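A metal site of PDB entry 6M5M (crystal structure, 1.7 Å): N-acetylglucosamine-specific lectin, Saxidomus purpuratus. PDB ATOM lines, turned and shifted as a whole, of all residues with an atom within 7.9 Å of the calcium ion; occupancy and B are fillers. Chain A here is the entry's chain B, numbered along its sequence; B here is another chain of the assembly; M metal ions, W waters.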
ATOM      1  N   PHE A  35       8.766 -16.044  17.306  1.00  0.00           N
ATOM      2  CA  PHE A  35       9.823 -17.040  17.561  1.00  0.00           C
ATOM      3  C   PHE A  35      10.987 -16.896  16.591  1.00  0.00           C
ATOM      4  O   PHE A  35      10.749 -16.812  15.399  1.00  0.00           O
ATOM      5  CB  PHE A  35       9.338 -18.483  17.412  1.00  0.00           C
ATOM      6  CG  PHE A  35      10.446 -19.441  17.709  1.00  0.00           C
ATOM      7  CD1 PHE A  35      10.806 -19.718  19.025  1.00  0.00           C
ATOM      8  CD2 PHE A  35      11.218 -19.992  16.686  1.00  0.00           C
ATOM      9  CE1 PHE A  35      11.849 -20.578  19.316  1.00  0.00           C
ATOM     10  CE2 PHE A  35      12.270 -20.849  16.981  1.00  0.00           C
ATOM     11  CZ  PHE A  35      12.590 -21.133  18.290  1.00  0.00           C
ATOM     12  N   GLY A  36      12.228 -16.959  17.076  1.00  0.00           N
ATOM     13  CA  GLY A  36      13.402 -17.069  16.195  1.00  0.00           C
ATOM     14  C   GLY A  36      13.392 -16.047  15.068  1.00  0.00           C
ATOM     15  O   GLY A  36      13.702 -16.402  13.909  1.00  0.00           O
ATOM     16  N   GLY A  37      13.038 -14.808  15.369  1.00  0.00           N
ATOM     17  CA  GLY A  37      13.076 -13.705  14.379  1.00  0.00           C
ATOM     18  C   GLY A  37      12.003 -13.838  13.308  1.00  0.00           C
ATOM     19  O   GLY A  37      12.106 -13.196  12.225  1.00  0.00           O
ATOM     20  N   SER A  38      10.951 -14.583  13.608  1.00  0.00           N
ATOM     21  CA  SER A  38       9.764 -14.724  12.748  1.00  0.00           C
ATOM     22  C   SER A  38       8.506 -14.469  13.571  1.00  0.00           C
ATOM     23  O   SER A  38       8.537 -14.754  14.816  1.00  0.00           O
ATOM     24  CB  SER A  38       9.752 -16.110  12.138  1.00  0.00           C
ATOM     25  OG  SER A  38      10.710 -16.170  11.094  1.00  0.00           O
ATOM     26  N   TYR A  40       4.468 -15.720  13.492  1.00  0.00           N
ATOM     27  CA  TYR A  40       3.670 -16.858  12.990  1.00  0.00           C
ATOM     28  C   TYR A  40       2.186 -16.645  13.285  1.00  0.00           C
ATOM     29  O   TYR A  40       1.805 -16.262  14.434  1.00  0.00           O
ATOM     30  CB  TYR A  40       4.160 -18.150  13.631  1.00  0.00           C
ATOM     31  CG  TYR A  40       5.615 -18.457  13.382  1.00  0.00           C
ATOM     32  CD1 TYR A  40       6.620 -17.898  14.138  1.00  0.00           C
ATOM     33  CD2 TYR A  40       5.980 -19.329  12.373  1.00  0.00           C
ATOM     34  CE1 TYR A  40       7.954 -18.179  13.893  1.00  0.00           C
ATOM     35  CE2 TYR A  40       7.309 -19.626  12.124  1.00  0.00           C
ATOM     36  CZ  TYR A  40       8.301 -19.072  12.891  1.00  0.00           C
ATOM     37  OH  TYR A  40       9.603 -19.341  12.630  1.00  0.00           O
ATOM     38  N   LEU A  63       2.973 -19.105   3.539  1.00  0.00           N
ATOM     39  CA  LEU A  63       2.960 -20.408   4.235  1.00  0.00           C
ATOM     40  C   LEU A  63       4.350 -20.647   4.816  1.00  0.00           C
ATOM     41  O   LEU A  63       5.347 -20.278   4.205  1.00  0.00           O
ATOM     42  CB  LEU A  63       2.522 -21.483   3.240  1.00  0.00           C
ATOM     43  CG  LEU A  63       1.021 -21.553   2.994  1.00  0.00           C
ATOM     44  CD1 LEU A  63       0.715 -22.459   1.837  1.00  0.00           C
ATOM     45  CD2 LEU A  63       0.295 -22.040   4.252  1.00  0.00           C
ATOM     46  N   VAL A  64       4.405 -21.139   6.033  1.00  0.00           N
ATOM     47  CA  VAL A  64       5.672 -21.171   6.798  1.00  0.00           C
ATOM     48  C   VAL A  64       6.708 -22.029   6.083  1.00  0.00           C
ATOM     49  O   VAL A  64       6.363 -22.990   5.414  1.00  0.00           O
ATOM     50  CB  VAL A  64       5.430 -21.726   8.201  1.00  0.00           C
ATOM     51  CG1 VAL A  64       4.957 -23.161   8.138  1.00  0.00           C
ATOM     52  CG2 VAL A  64       6.679 -21.601   9.026  1.00  0.00           C
ATOM     53  N   THR A  65       7.966 -21.643   6.244  1.00  0.00           N
ATOM     54  CA  THR A  65       9.176 -22.379   5.739  1.00  0.00           C
ATOM     55  C   THR A  65      10.030 -22.656   6.973  1.00  0.00           C
ATOM     56  O   THR A  65      10.171 -21.732   7.821  1.00  0.00           O
ATOM     57  CB  THR A  65       9.890 -21.586   4.636  1.00  0.00           C
ATOM     58  OG1 THR A  65      10.329 -20.326   5.157  1.00  0.00           O
ATOM     59  CG2 THR A  65       9.027 -21.357   3.409  1.00  0.00           C
ATOM     60  N   VAL A  66      10.524 -23.889   7.131  1.00  0.00           N
ATOM     61  CA  VAL A  66      11.175 -24.371   8.381  1.00  0.00           C
ATOM     62  C   VAL A  66      12.628 -24.691   8.055  1.00  0.00           C
ATOM     63  O   VAL A  66      12.916 -25.727   7.425  1.00  0.00           O
ATOM     64  CB  VAL A  66      10.396 -25.568   8.941  1.00  0.00           C
ATOM     65  CG1 VAL A  66      10.836 -25.940  10.343  1.00  0.00           C
ATOM     66  CG2 VAL A  66       8.893 -25.286   8.905  1.00  0.00           C
ATOM     67  N   GLU A  67      13.526 -23.831   8.505  1.00  0.00           N
ATOM     68  CA  GLU A  67      14.940 -23.846   8.029  1.00  0.00           C
ATOM     69  C   GLU A  67      15.824 -24.615   9.013  1.00  0.00           C
ATOM     70  O   GLU A  67      16.948 -24.964   8.607  1.00  0.00           O
ATOM     71  CB  GLU A  67      15.368 -22.405   7.796  1.00  0.00           C
ATOM     72  CG  GLU A  67      14.807 -21.830   6.482  1.00  0.00           C
ATOM     73  CD  GLU A  67      13.488 -21.070   6.637  1.00  0.00           C
ATOM     74  OE1 GLU A  67      13.090 -20.812   7.794  1.00  0.00           O
ATOM     75  OE2 GLU A  67      12.884 -20.720   5.601  1.00  0.00           O
ATOM     76  N   CYS A  68      15.358 -24.854  10.241  1.00  0.00           N
ATOM     77  CA  CYS A  68      16.158 -25.467  11.317  1.00  0.00           C
ATOM     78  C   CYS A  68      15.289 -26.192  12.352  1.00  0.00           C
ATOM     79  O   CYS A  68      14.039 -25.989  12.397  1.00  0.00           O
ATOM     80  CB  CYS A  68      16.968 -24.399  12.044  1.00  0.00           C
ATOM     81  SG  CYS A  68      15.923 -23.251  12.988  1.00  0.00           S
ATOM     82  N   GLU A  71      12.991 -24.190  14.966  1.00  0.00           N
ATOM     83  CA  GLU A  71      11.723 -23.699  14.365  1.00  0.00           C
ATOM     84  C   GLU A  71      10.732 -24.855  14.280  1.00  0.00           C
ATOM     85  O   GLU A  71       9.556 -24.632  14.542  1.00  0.00           O
ATOM     86  CB  GLU A  71      11.997 -23.051  13.007  1.00  0.00           C
ATOM     87  CG  GLU A  71      10.803 -22.281  12.435  1.00  0.00           C
ATOM     88  CD  GLU A  71      11.127 -21.625  11.116  1.00  0.00           C
ATOM     89  OE1 GLU A  71      12.107 -22.063  10.505  1.00  0.00           O
ATOM     90  OE2 GLU A  71      10.396 -20.668  10.663  1.00  0.00           O
ATOM     91  N   ILE A  75       7.133 -24.978  16.297  1.00  0.00           N
ATOM     92  CA  ILE A  75       5.843 -25.346  15.637  1.00  0.00           C
ATOM     93  C   ILE A  75       5.184 -26.536  16.354  1.00  0.00           C
ATOM     94  O   ILE A  75       3.984 -26.487  16.631  1.00  0.00           O
ATOM     95  CB  ILE A  75       6.015 -25.598  14.130  1.00  0.00           C
ATOM     96  CG1 ILE A  75       6.458 -24.325  13.410  1.00  0.00           C
ATOM     97  CG2 ILE A  75       4.723 -26.125  13.530  1.00  0.00           C
ATOM     98  CD1 ILE A  75       7.041 -24.536  12.055  1.00  0.00           C
ATOM     99  N   TRP A 103      10.733 -25.800  -0.642  1.00  0.00           N
ATOM    100  CA  TRP A 103       9.888 -24.667  -0.197  1.00  0.00           C
ATOM    101  C   TRP A 103       9.323 -23.917  -1.415  1.00  0.00           C
ATOM    102  O   TRP A 103       9.912 -23.952  -2.537  1.00  0.00           O
ATOM    103  CB  TRP A 103      10.654 -23.778   0.798  1.00  0.00           C
ATOM    104  CG  TRP A 103      11.156 -24.476   2.019  1.00  0.00           C
ATOM    105  CD1 TRP A 103      12.466 -24.624   2.387  1.00  0.00           C
ATOM    106  CD2 TRP A 103      10.397 -25.147   3.035  1.00  0.00           C
ATOM    107  NE1 TRP A 103      12.576 -25.373   3.536  1.00  0.00           N
ATOM    108  CE2 TRP A 103      11.308 -25.717   3.942  1.00  0.00           C
ATOM    109  CE3 TRP A 103       9.041 -25.389   3.212  1.00  0.00           C
ATOM    110  CZ2 TRP A 103      10.912 -26.453   5.066  1.00  0.00           C
ATOM    111  CZ3 TRP A 103       8.635 -26.083   4.323  1.00  0.00           C
ATOM    112  CH2 TRP A 103       9.558 -26.618   5.224  1.00  0.00           C
ATOM    113  N   GLU A 154       3.823 -17.261   7.959  1.00  0.00           N
ATOM    114  CA  GLU A 154       5.066 -16.728   8.568  1.00  0.00           C
ATOM    115  C   GLU A 154       5.429 -15.388   7.915  1.00  0.00           C
ATOM    116  O   GLU A 154       5.450 -15.340   6.684  1.00  0.00           O
ATOM    117  CB  GLU A 154       6.165 -17.789   8.410  1.00  0.00           C
ATOM    118  CG  GLU A 154       7.486 -17.372   9.064  1.00  0.00           C
ATOM    119  CD  GLU A 154       8.710 -18.188   8.664  1.00  0.00           C
ATOM    120  OE1 GLU A 154       8.609 -18.982   7.673  1.00  0.00           O
ATOM    121  OE2 GLU A 154       9.800 -17.963   9.305  1.00  0.00           O
ATOM    122  N   ILE A 155       5.818 -14.400   8.720  1.00  0.00           N
ATOM    123  CA  ILE A 155       6.480 -13.134   8.304  1.00  0.00           C
ATOM    124  C   ILE A 155       7.878 -13.192   8.941  1.00  0.00           C
ATOM    125  O   ILE A 155       7.934 -13.296  10.195  1.00  0.00           O
ATOM    126  CB  ILE A 155       5.669 -11.885   8.759  1.00  0.00           C
ATOM    127  CG1 ILE A 155       4.207 -11.937   8.319  1.00  0.00           C
ATOM    128  CG2 ILE A 155       6.333 -10.602   8.257  1.00  0.00           C
ATOM    129  CD1 ILE A 155       3.290 -10.918   9.017  1.00  0.00           C
ATOM    130  N   ASP A 156       8.954 -13.195   8.141  1.00  0.00           N
ATOM    131  CA  ASP A 156      10.337 -13.368   8.677  1.00  0.00           C
ATOM    132  C   ASP A 156      11.161 -12.089   8.453  1.00  0.00           C
ATOM    133  O   ASP A 156      12.346 -12.073   8.865  1.00  0.00           O
ATOM    134  CB  ASP A 156      10.946 -14.686   8.167  1.00  0.00           C
ATOM    135  CG  ASP A 156      11.304 -14.687   6.682  1.00  0.00           C
ATOM    136  OD1 ASP A 156      11.066 -13.651   6.009  1.00  0.00           O
ATOM    137  OD2 ASP A 156      11.852 -15.727   6.204  1.00  0.00           O
ATOM    138  N   LYS B  24      17.750 -18.998  10.502  1.00  0.00           N
ATOM    139  CA  LYS B  24      17.925 -17.821   9.622  1.00  0.00           C
ATOM    140  C   LYS B  24      18.435 -16.603  10.397  1.00  0.00           C
ATOM    141  O   LYS B  24      19.001 -15.739   9.750  1.00  0.00           O
ATOM    142  CB  LYS B  24      16.599 -17.409   8.978  1.00  0.00           C
ATOM    143  CG  LYS B  24      16.242 -18.134   7.696  1.00  0.00           C
ATOM    144  CD  LYS B  24      15.184 -17.429   6.860  1.00  0.00           C
ATOM    145  CE  LYS B  24      15.657 -16.112   6.267  1.00  0.00           C
ATOM    146  NZ  LYS B  24      14.721 -15.630   5.229  1.00  0.00           N
HETATM  147 CA    CA M   1      11.103 -19.856   8.757  1.00  0.00          CA
HETATM  148  O   HOH W   1      12.738 -18.670   9.875  1.00  0.00           O
HETATM  149  O   HOH W   2      11.609 -18.457   6.927  1.00  0.00           O
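The side-chain hydroxyl of Tyr 40 lies close to the side-chain carboxylate of Glu 71 (2.5 Å). The side-chain sulfur (SG) of Cys 68 sits at hydrogen-bond distance from the backbone NH (N) of Glu 71. The side-chain carboxylate (OE2) of Glu 154 lies close to the side-chain hydroxyl (OG) of Ser 38, at 2.7 Å.
Within 4 Å of the calcium ion: Thr 65, Glu 67, Glu 71 and Glu 154. Along chain A the residues within 4 Å of the calcium ion span positions 65 to 154.
The calcium ion is bound by OE2 of Glu 71 (2.2 Å), O of Thr 65 (2.3 Å), water W1 (2.3 Å), water W2 (2.4 Å), OE2 of Glu 154 (2.4 Å), OE1 of Glu 67 (2.4 Å) and OE1 of Glu 154 (2.9 Å). The calcium ion has seven donor atoms within binding distance. Slightly farther from the calcium ion lies OE1 of Glu 71 (3.0 Å).
Water W2 lies within hydrogen-bond range of OD2 of Asp 156 (2.8 Å), OG1 of Thr 65 (2.9 Å) and OE2 of Glu 67 (2.9 Å).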
